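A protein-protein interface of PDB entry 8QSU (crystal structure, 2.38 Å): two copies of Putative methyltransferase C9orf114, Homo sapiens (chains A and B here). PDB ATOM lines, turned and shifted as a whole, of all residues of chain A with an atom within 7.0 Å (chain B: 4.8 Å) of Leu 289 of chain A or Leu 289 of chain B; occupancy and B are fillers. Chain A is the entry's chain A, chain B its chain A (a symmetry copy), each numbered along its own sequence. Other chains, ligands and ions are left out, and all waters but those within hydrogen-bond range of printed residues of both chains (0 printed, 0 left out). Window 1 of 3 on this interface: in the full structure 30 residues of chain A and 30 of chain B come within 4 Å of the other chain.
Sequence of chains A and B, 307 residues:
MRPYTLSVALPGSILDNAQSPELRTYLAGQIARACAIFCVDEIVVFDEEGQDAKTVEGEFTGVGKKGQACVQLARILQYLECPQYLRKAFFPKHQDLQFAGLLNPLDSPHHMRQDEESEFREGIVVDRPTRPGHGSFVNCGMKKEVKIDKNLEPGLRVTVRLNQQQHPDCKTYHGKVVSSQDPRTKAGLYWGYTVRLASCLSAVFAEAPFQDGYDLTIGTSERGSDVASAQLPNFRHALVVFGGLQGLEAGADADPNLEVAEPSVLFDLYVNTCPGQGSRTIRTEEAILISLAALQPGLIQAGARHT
Of the printed residues of chain B, Ile 37 of chain A touches Glu 286 (3.9 Å) and Ile 290 (3.9 Å).
Phe 242 of chain A touches none of the printed residues of chain B.
Leu 289 of chain A touches just one residue of chain B: Leu 289 (3.8 Å).
Of the printed residues of chain A, Ile 37 of chain B touches Ile 282, Glu 286 and Ile 290.
Of the printed residues of chain A, Phe 38 of chain B touches Ile 290 (3.9 Å).
Leu 289 of chain B touches just one residue of chain A: Leu 289 (3.8 Å).
The nearest residue of chain B that does not touch Leu 289 of chain A is Ile 290 of chain B (4.1 Å).
The nearest residue of chain A that does not touch Leu 289 of chain B is Ile 290 of chain A (4.1 Å).
The nearest printed residue of chain A that does not touch Ile 37 of chain B is Arg 283 of chain A (5.8 Å).
OE2 of Glu 286 of chain B lies within salt-bridge range of NE of Arg 33 of chain A (2.8 Å).
Ile 37 of chain A touches Glu 286 of chain B, and with the chains exchanged Glu 286 of chain A touches Ile 37 of chain B.
Leu 289 of chain A touches its own counterpart, Leu 289 of chain B.
Ile 290 of chain A touches Ala 293 of chain B, and with the chains exchanged Ala 293 of chain A touches Ile 290 of chain B.
Ala 293 of chain A touches its own counterpart, Ala 293 of chain B.
Positions printed for both chains: 34, 37, 38, 285, 286, 287, 288, 289, 290, 291, 292 and 293.
Of the 12 pairs that touch across the chains among the printed residues, 10 have their exchanged pair printed and touching as well.
Ile 37 of chain A touches Glu 286 of chain B.
Ile 37 of chain A touches Ile 290 of chain B.
Ile 290 of chain B touches Phe 38 of chain A (CD1 to CE2, 3.8 Å).
Ile 37 of chain B touches Ile 282 of chain A.
Glu 286 of chain A touches Ile 37 of chain B (OE1 to CD1, 3.9 Å).
CD1 of Leu 289 of chain B touches CD1 of Leu 289 of chain A (3.8 Å).
CG2 of Ile 37 of chain B touches CD1 of Ile 290 of chain A, at 3.9 Å.
Ile 290 of chain A touches Ala 293 of chain B (O to CB, 3.9 Å).
Ile 290 of chain B touches Ala 293 of chain A (O to CB, 3.9 Å).
CB of Ala 293 of chain B touches CB of Ala 293 of chain A, 3.8 Å away.
Hydrophobic or aromatic side chains of chain A that line the printed part of chain B: Ile 37, Phe 38, Ile 282, Leu 289, Ile 290 and Ala 293.
Printed residues of chain B that touch a printed residue of chain A: Ile 37, Phe 38, Glu 286, Leu 289, Ile 290 and Ala 293.
Among the printed residues, 12 pairs touch across the chains.
Among the printed residues, Asp or Glu carboxylates within 4 Å of a Lys or Arg side-chain nitrogen of the other chain: Arg 33 of chain A with Glu 286 of chain B.
The backbone NH (N) of Arg 283 of chain A is in hydrogen-bond range of the side-chain carboxylate (OE1) of Glu 286 of chain A, 2.9 Å away.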
ATOM      1  N   GLN A  30      26.911 -22.687  23.332  1.00  0.00           N
ATOM      2  CA  GLN A  30      26.348 -23.445  22.211  1.00  0.00           C
ATOM      3  C   GLN A  30      27.102 -23.152  20.937  1.00  0.00           C
ATOM      4  O   GLN A  30      27.165 -24.013  20.056  1.00  0.00           O
ATOM      5  CB  GLN A  30      24.870 -23.112  21.944  1.00  0.00           C
ATOM      6  CG  GLN A  30      23.947 -23.234  23.109  1.00  0.00           C
ATOM      7  CD  GLN A  30      22.517 -22.955  22.697  1.00  0.00           C
ATOM      8  OE1 GLN A  30      21.969 -21.911  23.028  1.00  0.00           O
ATOM      9  NE2 GLN A  30      21.921 -23.875  21.934  1.00  0.00           N
ATOM     10  N   ARG A  33      30.340 -25.345  21.060  1.00  0.00           N
ATOM     11  CA  ARG A  33      30.104 -26.769  20.827  1.00  0.00           C
ATOM     12  C   ARG A  33      29.809 -27.037  19.362  1.00  0.00           C
ATOM     13  O   ARG A  33      30.317 -28.004  18.785  1.00  0.00           O
ATOM     14  CB  ARG A  33      28.969 -27.286  21.725  1.00  0.00           C
ATOM     15  CG  ARG A  33      29.463 -27.734  23.104  1.00  0.00           C
ATOM     16  CD  ARG A  33      28.454 -28.642  23.813  1.00  0.00           C
ATOM     17  NE  ARG A  33      28.121 -29.841  23.047  1.00  0.00           N
ATOM     18  CZ  ARG A  33      28.873 -30.929  23.002  1.00  0.00           C
ATOM     19  NH1 ARG A  33      30.021 -31.004  23.658  1.00  0.00           N
ATOM     20  NH2 ARG A  33      28.488 -31.954  22.249  1.00  0.00           N
ATOM     21  N   ALA A  34      29.033 -26.173  18.721  1.00  0.00           N
ATOM     22  CA  ALA A  34      28.722 -26.424  17.320  1.00  0.00           C
ATOM     23  C   ALA A  34      29.994 -26.400  16.468  1.00  0.00           C
ATOM     24  O   ALA A  34      30.174 -27.244  15.580  1.00  0.00           O
ATOM     25  CB  ALA A  34      27.700 -25.410  16.823  1.00  0.00           C
ATOM     26  N   CYS A  35      30.900 -25.459  16.744  1.00  0.00           N
ATOM     27  CA  CYS A  35      32.146 -25.409  15.987  1.00  0.00           C
ATOM     28  C   CYS A  35      33.057 -26.571  16.341  1.00  0.00           C
ATOM     29  O   CYS A  35      33.732 -27.115  15.461  1.00  0.00           O
ATOM     30  CB  CYS A  35      32.851 -24.071  16.220  1.00  0.00           C
ATOM     31  SG  CYS A  35      31.801 -22.690  15.727  1.00  0.00           S
ATOM     32  N   ILE A  37      32.018 -29.542  17.201  1.00  0.00           N
ATOM     33  CA  ILE A  37      31.469 -30.789  16.661  1.00  0.00           C
ATOM     34  C   ILE A  37      31.883 -30.970  15.211  1.00  0.00           C
ATOM     35  O   ILE A  37      32.178 -32.085  14.769  1.00  0.00           O
ATOM     36  CB  ILE A  37      29.938 -30.831  16.814  1.00  0.00           C
ATOM     37  CG1 ILE A  37      29.569 -30.853  18.290  1.00  0.00           C
ATOM     38  CG2 ILE A  37      29.343 -32.040  16.037  1.00  0.00           C
ATOM     39  CD1 ILE A  37      28.097 -30.412  18.544  1.00  0.00           C
ATOM     40  N   PHE A  38      31.937 -29.881  14.453  1.00  0.00           N
ATOM     41  CA  PHE A  38      32.268 -29.960  13.041  1.00  0.00           C
ATOM     42  C   PHE A  38      33.739 -29.706  12.771  1.00  0.00           C
ATOM     43  O   PHE A  38      34.106 -29.440  11.621  1.00  0.00           O
ATOM     44  CB  PHE A  38      31.396 -28.995  12.249  1.00  0.00           C
ATOM     45  CG  PHE A  38      30.002 -29.497  12.055  1.00  0.00           C
ATOM     46  CD1 PHE A  38      29.673 -30.246  10.936  1.00  0.00           C
ATOM     47  CD2 PHE A  38      29.036 -29.263  13.010  1.00  0.00           C
ATOM     48  CE1 PHE A  38      28.391 -30.720  10.755  1.00  0.00           C
ATOM     49  CE2 PHE A  38      27.745 -29.749  12.842  1.00  0.00           C
ATOM     50  CZ  PHE A  38      27.425 -30.482  11.713  1.00  0.00           C
ATOM     51  N   PHE A 242      27.848 -16.260   9.054  1.00  0.00           N
ATOM     52  CA  PHE A 242      26.505 -16.244   9.615  1.00  0.00           C
ATOM     53  C   PHE A 242      26.187 -14.842  10.109  1.00  0.00           C
ATOM     54  O   PHE A 242      27.050 -14.173  10.679  1.00  0.00           O
ATOM     55  CB  PHE A 242      26.391 -17.233  10.775  1.00  0.00           C
ATOM     56  CG  PHE A 242      26.623 -18.657  10.374  1.00  0.00           C
ATOM     57  CD1 PHE A 242      25.563 -19.451   9.922  1.00  0.00           C
ATOM     58  CD2 PHE A 242      27.884 -19.217  10.449  1.00  0.00           C
ATOM     59  CE1 PHE A 242      25.774 -20.767   9.545  1.00  0.00           C
ATOM     60  CE2 PHE A 242      28.103 -20.534  10.079  1.00  0.00           C
ATOM     61  CZ  PHE A 242      27.059 -21.303   9.610  1.00  0.00           C
ATOM     62  N   ILE A 282      15.447 -18.874  11.737  1.00  0.00           N
ATOM     63  CA  ILE A 282      16.390 -19.808  12.329  1.00  0.00           C
ATOM     64  C   ILE A 282      17.438 -18.979  13.053  1.00  0.00           C
ATOM     65  O   ILE A 282      18.146 -18.175  12.434  1.00  0.00           O
ATOM     66  CB  ILE A 282      17.033 -20.718  11.271  1.00  0.00           C
ATOM     67  CG1 ILE A 282      15.942 -21.448  10.474  1.00  0.00           C
ATOM     68  CG2 ILE A 282      17.965 -21.710  11.923  1.00  0.00           C
ATOM     69  CD1 ILE A 282      16.465 -22.257   9.282  1.00  0.00           C
ATOM     70  N   ARG A 283      17.537 -19.163  14.359  1.00  0.00           N
ATOM     71  CA  ARG A 283      18.536 -18.428  15.109  1.00  0.00           C
ATOM     72  C   ARG A 283      19.937 -18.889  14.720  1.00  0.00           C
ATOM     73  O   ARG A 283      20.140 -20.002  14.206  1.00  0.00           O
ATOM     74  CB  ARG A 283      18.292 -18.600  16.601  1.00  0.00           C
ATOM     75  CG  ARG A 283      16.834 -18.373  16.953  1.00  0.00           C
ATOM     76  CD  ARG A 283      16.520 -18.967  18.301  1.00  0.00           C
ATOM     77  NE  ARG A 283      17.439 -18.450  19.306  1.00  0.00           N
ATOM     78  CZ  ARG A 283      17.244 -17.309  19.949  1.00  0.00           C
ATOM     79  NH1 ARG A 283      16.156 -16.586  19.743  1.00  0.00           N
ATOM     80  NH2 ARG A 283      18.156 -16.890  20.827  1.00  0.00           N
ATOM     81  N   THR A 284      20.906 -18.004  14.987  1.00  0.00           N
ATOM     82  CA  THR A 284      22.278 -18.199  14.529  1.00  0.00           C
ATOM     83  C   THR A 284      22.851 -19.506  15.055  1.00  0.00           C
ATOM     84  O   THR A 284      23.461 -20.280  14.308  1.00  0.00           O
ATOM     85  CB  THR A 284      23.169 -17.017  14.976  1.00  0.00           C
ATOM     86  OG1 THR A 284      22.672 -15.782  14.441  1.00  0.00           O
ATOM     87  CG2 THR A 284      24.594 -17.232  14.499  1.00  0.00           C
ATOM     88  N   GLU A 285      22.681 -19.763  16.353  1.00  0.00           N
ATOM     89  CA  GLU A 285      23.197 -20.999  16.919  1.00  0.00           C
ATOM     90  C   GLU A 285      22.483 -22.221  16.329  1.00  0.00           C
ATOM     91  O   GLU A 285      23.085 -23.290  16.212  1.00  0.00           O
ATOM     92  CB  GLU A 285      23.092 -20.951  18.442  1.00  0.00           C
ATOM     93  CG  GLU A 285      21.694 -21.210  19.038  1.00  0.00           C
ATOM     94  CD  GLU A 285      20.850 -19.965  19.172  1.00  0.00           C
ATOM     95  OE1 GLU A 285      21.372 -18.882  18.821  1.00  0.00           O
ATOM     96  OE2 GLU A 285      19.665 -20.077  19.625  1.00  0.00           O
ATOM     97  N   GLU A 286      21.224 -22.087  15.910  1.00  0.00           N
ATOM     98  CA  GLU A 286      20.602 -23.202  15.200  1.00  0.00           C
ATOM     99  C   GLU A 286      21.089 -23.254  13.762  1.00  0.00           C
ATOM    100  O   GLU A 286      21.342 -24.338  13.222  1.00  0.00           O
ATOM    101  CB  GLU A 286      19.066 -23.093  15.230  1.00  0.00           C
ATOM    102  CG  GLU A 286      18.474 -23.181  16.601  1.00  0.00           C
ATOM    103  CD  GLU A 286      17.185 -22.423  16.692  1.00  0.00           C
ATOM    104  OE1 GLU A 286      16.948 -21.583  15.789  1.00  0.00           O
ATOM    105  OE2 GLU A 286      16.425 -22.657  17.672  1.00  0.00           O
ATOM    106  N   ALA A 287      21.241 -22.087  13.135  1.00  0.00           N
ATOM    107  CA  ALA A 287      21.684 -22.053  11.746  1.00  0.00           C
ATOM    108  C   ALA A 287      23.056 -22.701  11.564  1.00  0.00           C
ATOM    109  O   ALA A 287      23.281 -23.368  10.551  1.00  0.00           O
ATOM    110  CB  ALA A 287      21.673 -20.620  11.244  1.00  0.00           C
ATOM    111  N   ILE A 288      23.963 -22.568  12.540  1.00  0.00           N
ATOM    112  CA  ILE A 288      25.307 -23.138  12.402  1.00  0.00           C
ATOM    113  C   ILE A 288      25.254 -24.669  12.323  1.00  0.00           C
ATOM    114  O   ILE A 288      25.816 -25.284  11.415  1.00  0.00           O
ATOM    115  CB  ILE A 288      26.212 -22.634  13.548  1.00  0.00           C
ATOM    116  CG1 ILE A 288      26.483 -21.132  13.357  1.00  0.00           C
ATOM    117  CG2 ILE A 288      27.574 -23.366  13.582  1.00  0.00           C
ATOM    118  CD1 ILE A 288      27.597 -20.551  14.227  1.00  0.00           C
ATOM    119  N   LEU A 289      24.568 -25.312  13.262  1.00  0.00           N
ATOM    120  CA  LEU A 289      24.441 -26.770  13.218  1.00  0.00           C
ATOM    121  C   LEU A 289      23.792 -27.249  11.913  1.00  0.00           C
ATOM    122  O   LEU A 289      24.273 -28.203  11.279  1.00  0.00           O
ATOM    123  CB  LEU A 289      23.653 -27.245  14.431  1.00  0.00           C
ATOM    124  CG  LEU A 289      24.337 -27.035  15.783  1.00  0.00           C
ATOM    125  CD1 LEU A 289      23.363 -27.273  16.918  1.00  0.00           C
ATOM    126  CD2 LEU A 289      25.483 -27.988  15.907  1.00  0.00           C
ATOM    127  N   ILE A 290      22.713 -26.582  11.484  1.00  0.00           N
ATOM    128  CA  ILE A 290      22.049 -26.958  10.238  1.00  0.00           C
ATOM    129  C   ILE A 290      22.953 -26.696   9.033  1.00  0.00           C
ATOM    130  O   ILE A 290      22.975 -27.468   8.067  1.00  0.00           O
ATOM    131  CB  ILE A 290      20.705 -26.210  10.102  1.00  0.00           C
ATOM    132  CG1 ILE A 290      19.794 -26.424  11.319  1.00  0.00           C
ATOM    133  CG2 ILE A 290      19.958 -26.647   8.841  1.00  0.00           C
ATOM    134  CD1 ILE A 290      18.427 -25.650  11.219  1.00  0.00           C
ATOM    135  N   SER A 291      23.673 -25.580   9.037  1.00  0.00           N
ATOM    136  CA  SER A 291      24.438 -25.219   7.849  1.00  0.00           C
ATOM    137  C   SER A 291      25.657 -26.108   7.707  1.00  0.00           C
ATOM    138  O   SER A 291      25.937 -26.629   6.620  1.00  0.00           O
ATOM    139  CB  SER A 291      24.831 -23.751   7.904  1.00  0.00           C
ATOM    140  OG  SER A 291      23.689 -22.961   7.652  1.00  0.00           O
ATOM    141  N   LEU A 292      26.369 -26.327   8.811  1.00  0.00           N
ATOM    142  CA  LEU A 292      27.574 -27.137   8.755  1.00  0.00           C
ATOM    143  C   LEU A 292      27.238 -28.578   8.425  1.00  0.00           C
ATOM    144  O   LEU A 292      27.948 -29.230   7.648  1.00  0.00           O
ATOM    145  CB  LEU A 292      28.338 -27.024  10.069  1.00  0.00           C
ATOM    146  CG  LEU A 292      28.881 -25.613  10.270  1.00  0.00           C
ATOM    147  CD1 LEU A 292      29.880 -25.546  11.442  1.00  0.00           C
ATOM    148  CD2 LEU A 292      29.508 -25.137   8.966  1.00  0.00           C
ATOM    149  N   ALA A 293      26.151 -29.092   9.001  1.00  0.00           N
ATOM    150  CA  ALA A 293      25.660 -30.398   8.587  1.00  0.00           C
ATOM    151  C   ALA A 293      25.361 -30.409   7.092  1.00  0.00           C
ATOM    152  O   ALA A 293      25.818 -31.299   6.371  1.00  0.00           O
ATOM    153  CB  ALA A 293      24.431 -30.774   9.411  1.00  0.00           C
ATOM    154  N   ALA A 294      24.642 -29.393   6.593  1.00  0.00           N
ATOM    155  CA  ALA A 294      24.231 -29.416   5.191  1.00  0.00           C
ATOM    156  C   ALA A 294      25.390 -29.210   4.231  1.00  0.00           C
ATOM    157  O   ALA A 294      25.245 -29.500   3.035  1.00  0.00           O
ATOM    158  CB  ALA A 294      23.157 -28.352   4.922  1.00  0.00           C
ATOM    159  N   LEU A 295      26.524 -28.715   4.717  1.00  0.00           N
ATOM    160  CA  LEU A 295      27.683 -28.442   3.882  1.00  0.00           C
ATOM    161  C   LEU A 295      28.811 -29.450   4.050  1.00  0.00           C
ATOM    162  O   LEU A 295      29.579 -29.644   3.119  1.00  0.00           O
ATOM    163  CB  LEU A 295      28.208 -27.038   4.184  1.00  0.00           C
ATOM    164  CG  LEU A 295      27.259 -25.913   3.751  1.00  0.00           C
ATOM    165  CD1 LEU A 295      27.615 -24.641   4.489  1.00  0.00           C
ATOM    166  CD2 LEU A 295      27.318 -25.683   2.240  1.00  0.00           C
ATOM    167  N   ALA B  34      13.634 -27.179  17.024  1.00  0.00           N
ATOM    168  CA  ALA B  34      14.280 -28.018  16.022  1.00  0.00           C
ATOM    169  C   ALA B  34      13.241 -28.796  15.212  1.00  0.00           C
ATOM    170  O   ALA B  34      13.357 -28.912  13.984  1.00  0.00           O
ATOM    171  CB  ALA B  34      15.279 -28.953  16.693  1.00  0.00           C
ATOM    172  N   ILE B  37      11.440 -26.376  12.887  1.00  0.00           N
ATOM    173  CA  ILE B  37      12.224 -25.892  11.747  1.00  0.00           C
ATOM    174  C   ILE B  37      12.172 -26.888  10.602  1.00  0.00           C
ATOM    175  O   ILE B  37      12.104 -26.506   9.430  1.00  0.00           O
ATOM    176  CB  ILE B  37      13.676 -25.591  12.163  1.00  0.00           C
ATOM    177  CG1 ILE B  37      13.697 -24.446  13.163  1.00  0.00           C
ATOM    178  CG2 ILE B  37      14.554 -25.303  10.911  1.00  0.00           C
ATOM    179  CD1 ILE B  37      15.019 -24.398  13.986  1.00  0.00           C
ATOM    180  N   PHE B  38      12.181 -28.178  10.917  1.00  0.00           N
ATOM    181  CA  PHE B  38      12.191 -29.205   9.890  1.00  0.00           C
ATOM    182  C   PHE B  38      10.802 -29.726   9.572  1.00  0.00           C
ATOM    183  O   PHE B  38      10.681 -30.793   8.958  1.00  0.00           O
ATOM    184  CB  PHE B  38      13.116 -30.343  10.303  1.00  0.00           C
ATOM    185  CG  PHE B  38      14.562 -30.008  10.127  1.00  0.00           C
ATOM    186  CD1 PHE B  38      15.213 -30.306   8.941  1.00  0.00           C
ATOM    187  CD2 PHE B  38      15.255 -29.356  11.125  1.00  0.00           C
ATOM    188  CE1 PHE B  38      16.545 -29.992   8.767  1.00  0.00           C
ATOM    189  CE2 PHE B  38      16.593 -29.025  10.953  1.00  0.00           C
ATOM    190  CZ  PHE B  38      17.236 -29.341   9.770  1.00  0.00           C
ATOM    191  N   GLU B 285      19.659 -32.531  21.723  1.00  0.00           N
ATOM    192  CA  GLU B 285      19.159 -31.344  21.048  1.00  0.00           C
ATOM    193  C   GLU B 285      20.111 -30.896  19.933  1.00  0.00           C
ATOM    194  O   GLU B 285      19.666 -30.335  18.930  1.00  0.00           O
ATOM    195  CB  GLU B 285      18.908 -30.237  22.070  1.00  0.00           C
ATOM    196  CG  GLU B 285      20.152 -29.479  22.575  1.00  0.00           C
ATOM    197  CD  GLU B 285      20.810 -30.120  23.773  1.00  0.00           C
ATOM    198  OE1 GLU B 285      20.272 -31.153  24.234  1.00  0.00           O
ATOM    199  OE2 GLU B 285      21.865 -29.587  24.248  1.00  0.00           O
ATOM    200  N   GLU B 286      21.412 -31.165  20.055  1.00  0.00           N
ATOM    201  CA  GLU B 286      22.291 -30.886  18.923  1.00  0.00           C
ATOM    202  C   GLU B 286      22.154 -31.967  17.864  1.00  0.00           C
ATOM    203  O   GLU B 286      22.144 -31.673  16.662  1.00  0.00           O
ATOM    204  CB  GLU B 286      23.760 -30.776  19.373  1.00  0.00           C
ATOM    205  CG  GLU B 286      24.030 -29.642  20.309  1.00  0.00           C
ATOM    206  CD  GLU B 286      25.178 -29.944  21.223  1.00  0.00           C
ATOM    207  OE1 GLU B 286      25.527 -31.146  21.328  1.00  0.00           O
ATOM    208  OE2 GLU B 286      25.715 -28.985  21.842  1.00  0.00           O
ATOM    209  N   ALA B 287      22.029 -33.221  18.297  1.00  0.00           N
ATOM    210  CA  ALA B 287      21.913 -34.318  17.343  1.00  0.00           C
ATOM    211  C   ALA B 287      20.694 -34.165  16.435  1.00  0.00           C
ATOM    212  O   ALA B 287      20.776 -34.495  15.249  1.00  0.00           O
ATOM    213  CB  ALA B 287      21.891 -35.641  18.089  1.00  0.00           C
ATOM    214  N   ILE B 288      19.580 -33.625  16.943  1.00  0.00           N
ATOM    215  CA  ILE B 288      18.369 -33.487  16.127  1.00  0.00           C
ATOM    216  C   ILE B 288      18.597 -32.524  14.955  1.00  0.00           C
ATOM    217  O   ILE B 288      18.323 -32.846  13.798  1.00  0.00           O
ATOM    218  CB  ILE B 288      17.179 -33.067  17.019  1.00  0.00           C
ATOM    219  CG1 ILE B 288      16.804 -34.235  17.947  1.00  0.00           C
ATOM    220  CG2 ILE B 288      15.929 -32.697  16.186  1.00  0.00           C
ATOM    221  CD1 ILE B 288      15.468 -34.091  18.674  1.00  0.00           C
ATOM    222  N   LEU B 289      19.114 -31.331  15.229  1.00  0.00           N
ATOM    223  CA  LEU B 289      19.397 -30.382  14.151  1.00  0.00           C
ATOM    224  C   LEU B 289      20.373 -30.963  13.120  1.00  0.00           C
ATOM    225  O   LEU B 289      20.151 -30.849  11.902  1.00  0.00           O
ATOM    226  CB  LEU B 289      19.932 -29.086  14.746  1.00  0.00           C
ATOM    227  CG  LEU B 289      18.940 -28.295  15.600  1.00  0.00           C
ATOM    228  CD1 LEU B 289      19.648 -27.196  16.364  1.00  0.00           C
ATOM    229  CD2 LEU B 289      17.900 -27.690  14.711  1.00  0.00           C
ATOM    230  N   ILE B 290      21.446 -31.612  13.589  1.00  0.00           N
ATOM    231  CA  ILE B 290      22.413 -32.216  12.674  1.00  0.00           C
ATOM    232  C   ILE B 290      21.786 -33.376  11.901  1.00  0.00           C
ATOM    233  O   ILE B 290      22.065 -33.581  10.713  1.00  0.00           O
ATOM    234  CB  ILE B 290      23.667 -32.674  13.449  1.00  0.00           C
ATOM    235  CG1 ILE B 290      24.294 -31.536  14.268  1.00  0.00           C
ATOM    236  CG2 ILE B 290      24.723 -33.240  12.499  1.00  0.00           C
ATOM    237  CD1 ILE B 290      25.560 -31.983  15.090  1.00  0.00           C
ATOM    238  N   SER B 291      20.972 -34.189  12.565  1.00  0.00           N
ATOM    239  CA  SER B 291      20.465 -35.387  11.907  1.00  0.00           C
ATOM    240  C   SER B 291      19.409 -35.028  10.880  1.00  0.00           C
ATOM    241  O   SER B 291      19.441 -35.516   9.743  1.00  0.00           O
ATOM    242  CB  SER B 291      19.920 -36.362  12.939  1.00  0.00           C
ATOM    243  OG  SER B 291      21.001 -36.955  13.625  1.00  0.00           O
ATOM    244  N   LEU B 292      18.491 -34.139  11.253  1.00  0.00           N
ATOM    245  CA  LEU B 292      17.421 -33.768  10.343  1.00  0.00           C
ATOM    246  C   LEU B 292      17.971 -33.020   9.144  1.00  0.00           C
ATOM    247  O   LEU B 292      17.528 -33.236   8.008  1.00  0.00           O
ATOM    248  CB  LEU B 292      16.370 -32.948  11.083  1.00  0.00           C
ATOM    249  CG  LEU B 292      15.652 -33.793  12.131  1.00  0.00           C
ATOM    250  CD1 LEU B 292      14.411 -33.073  12.693  1.00  0.00           C
ATOM    251  CD2 LEU B 292      15.293 -35.140  11.516  1.00  0.00           C
ATOM    252  N   ALA B 293      18.945 -32.139   9.376  1.00  0.00           N
ATOM    253  CA  ALA B 293      19.650 -31.528   8.259  1.00  0.00           C
ATOM    254  C   ALA B 293      20.282 -32.597   7.375  1.00  0.00           C
ATOM    255  O   ALA B 293      20.096 -32.587   6.156  1.00  0.00           O
ATOM    256  CB  ALA B 293      20.691 -30.541   8.782  1.00  0.00           C
